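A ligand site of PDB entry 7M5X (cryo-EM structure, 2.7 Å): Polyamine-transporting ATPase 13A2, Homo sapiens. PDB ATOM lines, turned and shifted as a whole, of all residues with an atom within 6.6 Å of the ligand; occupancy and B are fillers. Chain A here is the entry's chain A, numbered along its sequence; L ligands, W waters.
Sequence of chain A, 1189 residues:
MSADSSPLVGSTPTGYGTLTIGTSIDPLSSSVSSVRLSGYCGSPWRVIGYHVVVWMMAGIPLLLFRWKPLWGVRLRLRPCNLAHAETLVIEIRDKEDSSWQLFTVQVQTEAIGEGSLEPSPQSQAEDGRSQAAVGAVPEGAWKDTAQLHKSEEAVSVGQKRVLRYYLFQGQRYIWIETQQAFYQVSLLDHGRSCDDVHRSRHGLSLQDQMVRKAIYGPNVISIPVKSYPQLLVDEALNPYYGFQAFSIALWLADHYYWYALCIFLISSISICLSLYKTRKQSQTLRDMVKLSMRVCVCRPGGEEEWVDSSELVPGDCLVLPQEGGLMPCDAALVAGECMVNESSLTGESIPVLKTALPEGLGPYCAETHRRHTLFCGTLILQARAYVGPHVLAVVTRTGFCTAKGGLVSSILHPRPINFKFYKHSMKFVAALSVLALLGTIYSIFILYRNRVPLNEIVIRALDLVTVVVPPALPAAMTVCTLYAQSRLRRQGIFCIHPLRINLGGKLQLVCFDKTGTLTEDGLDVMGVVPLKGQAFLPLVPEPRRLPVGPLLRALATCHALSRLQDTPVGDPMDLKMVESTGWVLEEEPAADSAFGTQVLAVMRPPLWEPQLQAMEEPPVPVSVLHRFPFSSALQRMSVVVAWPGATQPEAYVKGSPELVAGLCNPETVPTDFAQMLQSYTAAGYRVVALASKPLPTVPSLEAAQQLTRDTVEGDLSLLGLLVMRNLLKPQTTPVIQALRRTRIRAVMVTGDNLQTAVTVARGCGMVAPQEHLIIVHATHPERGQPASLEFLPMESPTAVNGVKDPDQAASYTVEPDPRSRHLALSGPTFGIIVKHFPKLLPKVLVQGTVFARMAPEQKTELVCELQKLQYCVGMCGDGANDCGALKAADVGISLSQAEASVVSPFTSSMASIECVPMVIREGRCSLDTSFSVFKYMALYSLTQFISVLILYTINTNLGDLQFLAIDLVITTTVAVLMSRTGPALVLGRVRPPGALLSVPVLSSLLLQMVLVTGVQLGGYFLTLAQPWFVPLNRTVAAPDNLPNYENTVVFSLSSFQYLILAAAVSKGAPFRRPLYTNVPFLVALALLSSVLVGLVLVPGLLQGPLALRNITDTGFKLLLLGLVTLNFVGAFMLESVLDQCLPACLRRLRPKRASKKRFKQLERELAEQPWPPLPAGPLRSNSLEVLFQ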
ATOM      1  N   TRP A 251       7.161 -14.392  -8.896  1.00  0.00           N
ATOM      2  CA  TRP A 251       6.213 -14.392 -10.008  1.00  0.00           C
ATOM      3  C   TRP A 251       4.879 -15.017  -9.607  1.00  0.00           C
ATOM      4  O   TRP A 251       3.826 -14.542 -10.045  1.00  0.00           O
ATOM      5  CB  TRP A 251       6.825 -15.130 -11.192  1.00  0.00           C
ATOM      6  CG  TRP A 251       7.909 -14.362 -11.902  1.00  0.00           C
ATOM      7  CD1 TRP A 251       8.125 -13.013 -11.876  1.00  0.00           C
ATOM      8  CD2 TRP A 251       8.924 -14.917 -12.735  1.00  0.00           C
ATOM      9  NE1 TRP A 251       9.216 -12.697 -12.646  1.00  0.00           N
ATOM     10  CE2 TRP A 251       9.719 -13.847 -13.188  1.00  0.00           C
ATOM     11  CE3 TRP A 251       9.241 -16.207 -13.152  1.00  0.00           C
ATOM     12  CZ2 TRP A 251      10.817 -14.033 -14.023  1.00  0.00           C
ATOM     13  CZ3 TRP A 251      10.326 -16.391 -13.988  1.00  0.00           C
ATOM     14  CH2 TRP A 251      11.098 -15.308 -14.415  1.00  0.00           C
ATOM     15  N   ASP A 254       3.160 -12.444  -8.078  1.00  0.00           N
ATOM     16  CA  ASP A 254       2.772 -11.387  -9.011  1.00  0.00           C
ATOM     17  C   ASP A 254       1.895 -11.908 -10.138  1.00  0.00           C
ATOM     18  O   ASP A 254       1.770 -11.257 -11.177  1.00  0.00           O
ATOM     19  CB  ASP A 254       4.015 -10.701  -9.582  1.00  0.00           C
ATOM     20  CG  ASP A 254       3.716  -9.345 -10.183  1.00  0.00           C
ATOM     21  OD1 ASP A 254       2.902  -8.599  -9.591  1.00  0.00           O
ATOM     22  OD2 ASP A 254       4.285  -9.026 -11.247  1.00  0.00           O
ATOM     23  N   HIS A 255       1.287 -13.080  -9.956  1.00  0.00           N
ATOM     24  CA  HIS A 255       0.329 -13.651 -10.904  1.00  0.00           C
ATOM     25  C   HIS A 255       0.937 -13.981 -12.255  1.00  0.00           C
ATOM     26  O   HIS A 255       0.211 -14.144 -13.243  1.00  0.00           O
ATOM     27  CB  HIS A 255      -0.868 -12.716 -11.097  1.00  0.00           C
ATOM     28  CG  HIS A 255      -1.560 -12.338  -9.821  1.00  0.00           C
ATOM     29  ND1 HIS A 255      -0.964 -11.557  -8.867  1.00  0.00           N
ATOM     30  CD2 HIS A 255      -2.790 -12.641  -9.352  1.00  0.00           C
ATOM     31  CE1 HIS A 255      -1.801 -11.392  -7.858  1.00  0.00           C
ATOM     32  NE2 HIS A 255      -2.913 -12.034  -8.128  1.00  0.00           N
ATOM     33  N   TYR A 256       2.262 -14.099 -12.332  1.00  0.00           N
ATOM     34  CA  TYR A 256       2.943 -14.480 -13.578  1.00  0.00           C
ATOM     35  C   TYR A 256       3.265 -15.977 -13.525  1.00  0.00           C
ATOM     36  O   TYR A 256       4.419 -16.405 -13.425  1.00  0.00           O
ATOM     37  CB  TYR A 256       4.194 -13.623 -13.772  1.00  0.00           C
ATOM     38  CG  TYR A 256       4.718 -13.560 -15.187  1.00  0.00           C
ATOM     39  CD1 TYR A 256       3.881 -13.196 -16.236  1.00  0.00           C
ATOM     40  CD2 TYR A 256       6.040 -13.847 -15.468  1.00  0.00           C
ATOM     41  CE1 TYR A 256       4.360 -13.129 -17.525  1.00  0.00           C
ATOM     42  CE2 TYR A 256       6.519 -13.780 -16.757  1.00  0.00           C
ATOM     43  CZ  TYR A 256       5.678 -13.428 -17.785  1.00  0.00           C
ATOM     44  OH  TYR A 256       6.155 -13.359 -19.064  1.00  0.00           O
ATOM     45  N   TYR A 259       5.328 -18.377 -17.019  1.00  0.00           N
ATOM     46  CA  TYR A 259       6.777 -18.341 -17.179  1.00  0.00           C
ATOM     47  C   TYR A 259       7.480 -18.883 -15.943  1.00  0.00           C
ATOM     48  O   TYR A 259       8.527 -19.525 -16.064  1.00  0.00           O
ATOM     49  CB  TYR A 259       7.251 -16.922 -17.465  1.00  0.00           C
ATOM     50  CG  TYR A 259       8.616 -16.822 -18.128  1.00  0.00           C
ATOM     51  CD1 TYR A 259       8.924 -17.576 -19.254  1.00  0.00           C
ATOM     52  CD2 TYR A 259       9.581 -15.979 -17.625  1.00  0.00           C
ATOM     53  CE1 TYR A 259      10.157 -17.487 -19.861  1.00  0.00           C
ATOM     54  CE2 TYR A 259      10.822 -15.883 -18.221  1.00  0.00           C
ATOM     55  CZ  TYR A 259      11.106 -16.640 -19.339  1.00  0.00           C
ATOM     56  OH  TYR A 259      12.339 -16.550 -19.936  1.00  0.00           O
ATOM     57  N   GLU A 456       2.282  -3.196  -3.896  1.00  0.00           N
ATOM     58  CA  GLU A 456       2.535  -3.075  -5.329  1.00  0.00           C
ATOM     59  C   GLU A 456       3.929  -2.532  -5.603  1.00  0.00           C
ATOM     60  O   GLU A 456       4.612  -2.997  -6.515  1.00  0.00           O
ATOM     61  CB  GLU A 456       1.477  -2.174  -5.967  1.00  0.00           C
ATOM     62  CG  GLU A 456       0.070  -2.753  -5.954  1.00  0.00           C
ATOM     63  CD  GLU A 456      -0.066  -3.993  -6.814  1.00  0.00           C
ATOM     64  OE1 GLU A 456       0.647  -4.078  -7.846  1.00  0.00           O
ATOM     65  OE2 GLU A 456      -0.873  -4.878  -6.474  1.00  0.00           O
ATOM     66  N   ARG A 460       6.662  -4.612  -7.748  1.00  0.00           N
ATOM     67  CA  ARG A 460       7.198  -4.061  -8.993  1.00  0.00           C
ATOM     68  C   ARG A 460       8.704  -3.895  -8.908  1.00  0.00           C
ATOM     69  O   ARG A 460       9.434  -4.254  -9.847  1.00  0.00           O
ATOM     70  CB  ARG A 460       6.535  -2.718  -9.291  1.00  0.00           C
ATOM     71  CG  ARG A 460       5.026  -2.778  -9.469  1.00  0.00           C
ATOM     72  CD  ARG A 460       4.631  -2.861 -10.934  1.00  0.00           C
ATOM     73  NE  ARG A 460       5.115  -4.080 -11.562  1.00  0.00           N
ATOM     74  CZ  ARG A 460       4.620  -5.287 -11.343  1.00  0.00           C
ATOM     75  NH1 ARG A 460       3.601  -5.486 -10.517  1.00  0.00           N
ATOM     76  NH2 ARG A 460       5.148  -6.334 -11.975  1.00  0.00           N
ATOM     77  N   ASP A 463      10.356  -7.257  -9.111  1.00  0.00           N
ATOM     78  CA  ASP A 463      10.237  -7.840 -10.437  1.00  0.00           C
ATOM     79  C   ASP A 463      11.161  -7.163 -11.439  1.00  0.00           C
ATOM     80  O   ASP A 463      11.594  -7.792 -12.412  1.00  0.00           O
ATOM     81  CB  ASP A 463       8.792  -7.757 -10.907  1.00  0.00           C
ATOM     82  CG  ASP A 463       8.606  -8.315 -12.295  1.00  0.00           C
ATOM     83  OD1 ASP A 463       9.116  -9.418 -12.568  1.00  0.00           O
ATOM     84  OD2 ASP A 463       7.945  -7.647 -13.125  1.00  0.00           O
ATOM     85  N   THR A 466      14.297  -9.207 -11.617  1.00  0.00           N
ATOM     86  CA  THR A 466      14.208 -10.375 -12.489  1.00  0.00           C
ATOM     87  C   THR A 466      14.201  -9.961 -13.954  1.00  0.00           C
ATOM     88  O   THR A 466      14.697 -10.708 -14.806  1.00  0.00           O
ATOM     89  CB  THR A 466      12.939 -11.182 -12.171  1.00  0.00           C
ATOM     90  OG1 THR A 466      11.784 -10.398 -12.453  1.00  0.00           O
ATOM     91  CG2 THR A 466      12.932 -11.594 -10.708  1.00  0.00           C
ATOM     92  N   VAL A 467      13.639  -8.799 -14.271  1.00  0.00           N
ATOM     93  CA  VAL A 467      13.740  -8.283 -15.634  1.00  0.00           C
ATOM     94  C   VAL A 467      15.201  -8.023 -15.990  1.00  0.00           C
ATOM     95  O   VAL A 467      15.633  -8.314 -17.113  1.00  0.00           O
ATOM     96  CB  VAL A 467      12.892  -7.000 -15.784  1.00  0.00           C
ATOM     97  CG1 VAL A 467      13.204  -6.317 -17.111  1.00  0.00           C
ATOM     98  CG2 VAL A 467      11.420  -7.333 -15.695  1.00  0.00           C
ATOM     99  N   PRO A 471      16.508 -15.165 -15.567  1.00  0.00           N
ATOM    100  CA  PRO A 471      16.621 -16.493 -14.949  1.00  0.00           C
ATOM    101  C   PRO A 471      16.753 -17.632 -15.941  1.00  0.00           C
ATOM    102  O   PRO A 471      17.042 -18.753 -15.529  1.00  0.00           O
ATOM    103  CB  PRO A 471      15.320 -16.616 -14.134  1.00  0.00           C
ATOM    104  CG  PRO A 471      14.798 -15.227 -14.036  1.00  0.00           C
ATOM    105  CD  PRO A 471      15.185 -14.578 -15.309  1.00  0.00           C
ATOM    106  N   TYR A 940      18.165  -8.602 -24.850  1.00  0.00           N
ATOM    107  CA  TYR A 940      16.797  -8.954 -24.422  1.00  0.00           C
ATOM    108  C   TYR A 940      16.561  -8.420 -23.010  1.00  0.00           C
ATOM    109  O   TYR A 940      15.559  -7.755 -22.876  1.00  0.00           O
ATOM    110  CB  TYR A 940      16.513 -10.459 -24.519  1.00  0.00           C
ATOM    111  CG  TYR A 940      15.531 -10.976 -23.512  1.00  0.00           C
ATOM    112  CD1 TYR A 940      14.165 -10.811 -23.678  1.00  0.00           C
ATOM    113  CD2 TYR A 940      15.965 -11.656 -22.393  1.00  0.00           C
ATOM    114  CE1 TYR A 940      13.255 -11.288 -22.748  1.00  0.00           C
ATOM    115  CE2 TYR A 940      15.076 -12.128 -21.451  1.00  0.00           C
ATOM    116  CZ  TYR A 940      13.720 -11.959 -21.637  1.00  0.00           C
ATOM    117  OH  TYR A 940      12.858 -12.466 -20.717  1.00  0.00           O
ATOM    118  N   GLN A 944      14.395  -4.679 -22.454  1.00  0.00           N
ATOM    119  CA  GLN A 944      13.167  -4.863 -21.714  1.00  0.00           C
ATOM    120  C   GLN A 944      13.153  -3.970 -20.489  1.00  0.00           C
ATOM    121  O   GLN A 944      12.206  -3.198 -20.290  1.00  0.00           O
ATOM    122  CB  GLN A 944      13.010  -6.323 -21.306  1.00  0.00           C
ATOM    123  CG  GLN A 944      11.621  -6.714 -20.866  1.00  0.00           C
ATOM    124  CD  GLN A 944      11.537  -8.170 -20.459  1.00  0.00           C
ATOM    125  OE1 GLN A 944      12.536  -8.886 -20.456  1.00  0.00           O
ATOM    126  NE2 GLN A 944      10.333  -8.618 -20.113  1.00  0.00           N
ATOM    127  N   TYR A 952       7.110   2.570 -16.410  1.00  0.00           N
ATOM    128  CA  TYR A 952       7.070   2.863 -14.979  1.00  0.00           C
ATOM    129  C   TYR A 952       7.152   4.360 -14.721  1.00  0.00           C
ATOM    130  O   TYR A 952       6.729   4.824 -13.657  1.00  0.00           O
ATOM    131  CB  TYR A 952       8.210   2.130 -14.258  1.00  0.00           C
ATOM    132  CG  TYR A 952       7.912   0.706 -13.840  1.00  0.00           C
ATOM    133  CD1 TYR A 952       6.988  -0.068 -14.529  1.00  0.00           C
ATOM    134  CD2 TYR A 952       8.569   0.148 -12.759  1.00  0.00           C
ATOM    135  CE1 TYR A 952       6.733  -1.364 -14.140  1.00  0.00           C
ATOM    136  CE2 TYR A 952       8.313  -1.149 -12.370  1.00  0.00           C
ATOM    137  CZ  TYR A 952       7.399  -1.902 -13.061  1.00  0.00           C
ATOM    138  OH  TYR A 952       7.137  -3.191 -12.673  1.00  0.00           O
ATOM    139  N   ASN A 957       2.588  -0.482 -17.038  1.00  0.00           N
ATOM    140  CA  ASN A 957       3.403  -1.676 -17.205  1.00  0.00           C
ATOM    141  C   ASN A 957       3.013  -2.333 -18.514  1.00  0.00           C
ATOM    142  O   ASN A 957       1.987  -1.986 -19.117  1.00  0.00           O
ATOM    143  CB  ASN A 957       3.232  -2.621 -16.015  1.00  0.00           C
ATOM    144  CG  ASN A 957       4.305  -3.685 -15.934  1.00  0.00           C
ATOM    145  OD1 ASN A 957       5.396  -3.527 -16.474  1.00  0.00           O
ATOM    146  ND2 ASN A 957       4.002  -4.783 -15.259  1.00  0.00           N
ATOM    147  N   GLY A 959       2.086  -5.637 -19.335  1.00  0.00           N
ATOM    148  CA  GLY A 959       0.904  -6.481 -19.277  1.00  0.00           C
ATOM    149  C   GLY A 959       1.342  -7.932 -19.236  1.00  0.00           C
ATOM    150  O   GLY A 959       2.374  -8.305 -19.804  1.00  0.00           O
ATOM    151  N   ASP A 960       0.543  -8.758 -18.567  1.00  0.00           N
ATOM    152  CA  ASP A 960       0.924 -10.157 -18.367  1.00  0.00           C
ATOM    153  C   ASP A 960       1.053 -10.883 -19.699  1.00  0.00           C
ATOM    154  O   ASP A 960       2.026 -11.605 -19.941  1.00  0.00           O
ATOM    155  CB  ASP A 960      -0.103 -10.858 -17.476  1.00  0.00           C
ATOM    156  CG  ASP A 960      -0.120 -10.298 -16.071  1.00  0.00           C
ATOM    157  OD1 ASP A 960      -0.834  -9.305 -15.830  1.00  0.00           O
ATOM    158  OD2 ASP A 960       0.584 -10.861 -15.198  1.00  0.00           O
ATOM    159  N   PHE A 963       4.033  -9.572 -21.496  1.00  0.00           N
ATOM    160  CA  PHE A 963       5.243 -10.110 -20.890  1.00  0.00           C
ATOM    161  C   PHE A 963       5.489 -11.537 -21.340  1.00  0.00           C
ATOM    162  O   PHE A 963       6.619 -11.919 -21.623  1.00  0.00           O
ATOM    163  CB  PHE A 963       5.145 -10.043 -19.359  1.00  0.00           C
ATOM    164  CG  PHE A 963       5.773  -8.813 -18.756  1.00  0.00           C
ATOM    165  CD1 PHE A 963       7.129  -8.574 -18.879  1.00  0.00           C
ATOM    166  CD2 PHE A 963       5.001  -7.911 -18.055  1.00  0.00           C
ATOM    167  CE1 PHE A 963       7.707  -7.456 -18.329  1.00  0.00           C
ATOM    168  CE2 PHE A 963       5.577  -6.791 -17.485  1.00  0.00           C
ATOM    169  CZ  PHE A 963       6.927  -6.560 -17.628  1.00  0.00           C
ATOM    170  N   ASP A 967       8.650 -12.928 -23.371  1.00  0.00           N
ATOM    171  CA  ASP A 967       9.554 -13.829 -22.659  1.00  0.00           C
ATOM    172  C   ASP A 967       9.440 -15.259 -23.161  1.00  0.00           C
ATOM    173  O   ASP A 967      10.439 -15.971 -23.259  1.00  0.00           O
ATOM    174  CB  ASP A 967       9.274 -13.769 -21.169  1.00  0.00           C
ATOM    175  CG  ASP A 967       9.464 -12.391 -20.582  1.00  0.00           C
ATOM    176  OD1 ASP A 967      10.277 -11.621 -21.141  1.00  0.00           O
ATOM    177  OD2 ASP A 967       8.812 -12.072 -19.569  1.00  0.00           O
ATOM    178  N   PRO A1039      -1.891  -2.379 -14.529  1.00  0.00           N
ATOM    179  CA  PRO A1039      -2.587  -3.259 -15.473  1.00  0.00           C
ATOM    180  C   PRO A1039      -3.966  -2.756 -15.871  1.00  0.00           C
ATOM    181  O   PRO A1039      -4.435  -3.102 -16.971  1.00  0.00           O
ATOM    182  CB  PRO A1039      -2.672  -4.582 -14.717  1.00  0.00           C
ATOM    183  CG  PRO A1039      -2.740  -4.186 -13.301  1.00  0.00           C
ATOM    184  CD  PRO A1039      -1.885  -2.954 -13.167  1.00  0.00           C
ATOM    185  N   ASP A1040      -4.627  -1.972 -15.033  1.00  0.00           N
ATOM    186  CA  ASP A1040      -5.943  -1.439 -15.326  1.00  0.00           C
ATOM    187  C   ASP A1040      -5.889  -0.188 -16.199  1.00  0.00           C
ATOM    188  O   ASP A1040      -6.950   0.313 -16.600  1.00  0.00           O
ATOM    189  CB  ASP A1040      -6.691  -1.137 -14.028  1.00  0.00           C
ATOM    190  CG  ASP A1040      -7.255  -2.386 -13.376  1.00  0.00           C
ATOM    191  OD1 ASP A1040      -6.905  -3.504 -13.819  1.00  0.00           O
ATOM    192  OD2 ASP A1040      -8.039  -2.254 -12.418  1.00  0.00           O
HETATM  193  N1  LIG L   1      10.715 -11.089 -17.463  1.00  0.00           N
HETATM  194  C1  LIG L   1      10.166 -11.200 -16.066  1.00  0.00           C
HETATM  195  C2  LIG L   1       9.180 -10.048 -15.843  1.00  0.00           C
HETATM  196  C3  LIG L   1       7.808 -10.554 -15.530  1.00  0.00           C
HETATM  197  N2  LIG L   1       6.910  -9.389 -15.197  1.00  0.00           N
HETATM  198  C4  LIG L   1       5.516  -9.926 -15.086  1.00  0.00           C
HETATM  199  C5  LIG L   1       4.717  -8.838 -14.429  1.00  0.00           C
HETATM  200  C6  LIG L   1       3.376  -9.464 -14.200  1.00  0.00           C
HETATM  201  C7  LIG L   1       2.527  -8.321 -13.717  1.00  0.00           C
HETATM  202  N3  LIG L   1       1.362  -8.981 -13.049  1.00  0.00           N
HETATM  203  C8  LIG L   1       0.508  -7.882 -12.511  1.00  0.00           C
HETATM  204  C9  LIG L   1      -0.697  -8.554 -11.887  1.00  0.00           C
HETATM  205  C10 LIG L   1      -1.828  -7.548 -11.907  1.00  0.00           C
HETATM  206  N4  LIG L   1      -3.064  -8.196 -11.299  1.00  0.00           N
HETATM  207  O   HOH W   1      13.571 -12.166 -17.782  1.00  0.00           O
HETATM  208  O   HOH W   2       1.201  -4.480 -12.659  1.00  0.00           O
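OD2 of Asp 967 is in salt-bridge range of N1 of the ligand. The side-chain carboxylate of Asp 960 lies within salt-bridge range of a nitrogen (N3) of the ligand (3.0 Å). N3 of the ligand lies within hydrogen-bond range of O of Asp 254, 3.0 Å away. OD2 of Asp 254 lies within salt-bridge range of N3 of the ligand (3.4 Å). The side-chain carboxylate (OD2) of Asp 463 is in salt-bridge range of a nitrogen (N2) of the ligand.
Water W1 lies within hydrogen-bond range of OH of Tyr 940 (3.0 Å), N1 of the ligand (3.1 Å) and O of Thr 466 (3.5 Å).
The side-chain hydroxyl (OH) of Tyr 256 is in hydrogen-bond range of the backbone carbonyl oxygen (O) of Phe 963 (3.0 Å). The side-chain carboxylate (OD2) of Asp 254 is in salt-bridge range of the guanidinium group (NH2) of Arg 460. OD2 of Asp 463 lies within salt-bridge range of NH2 of Arg 460 (3.3 Å). The indole nitrogen of Trp 251 sits at hydrogen-bond distance from the side-chain hydroxyl of Thr 466 (3.5 Å). The side-chain carboxylate of Asp 967 is in hydrogen-bond range of the side-chain hydroxyl of Tyr 256 (3.0 Å). The backbone carbonyl oxygen (O) of Trp 251 lies within hydrogen-bond range of the backbone NH (N) of Tyr 256 (2.8 Å). The side-chain carboxylate of Asp 967 sits at hydrogen-bond distance from the side-chain hydroxyl of Tyr 940, 2.7 Å away. The side-chain carboxylate (OD1) of Asp 967 is in hydrogen-bond range of the side-chain amide nitrogen (NE2) of Gln 944 (3.2 Å).
CZ2 of Trp 251 touches C1 of the ligand, at 3.6 Å. CE2 of Tyr 256 touches C3 of the ligand, at 3.7 Å. NH2 of Arg 460 touches C5 of the ligand (3.5 Å). Val 467 touches the ligand (CG2 to C2, 3.5 Å). Gln 944 touches the ligand (NE2 to N1, 3.6 Å). CD2 of Phe 963 touches C4 of the ligand, 3.6 Å away. Pro 1039 touches the ligand (CG to C10, 3.8 Å). Hydrophobic or aromatic side chains that line the ligand: Trp 251, Tyr 256, Val 467, Phe 963 and Pro 1039. Of the 21 residues printed, 11 come within 4 Å of the ligand. The nearest printed residue that does not touch the ligand is Thr 466 (4.04 Å).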
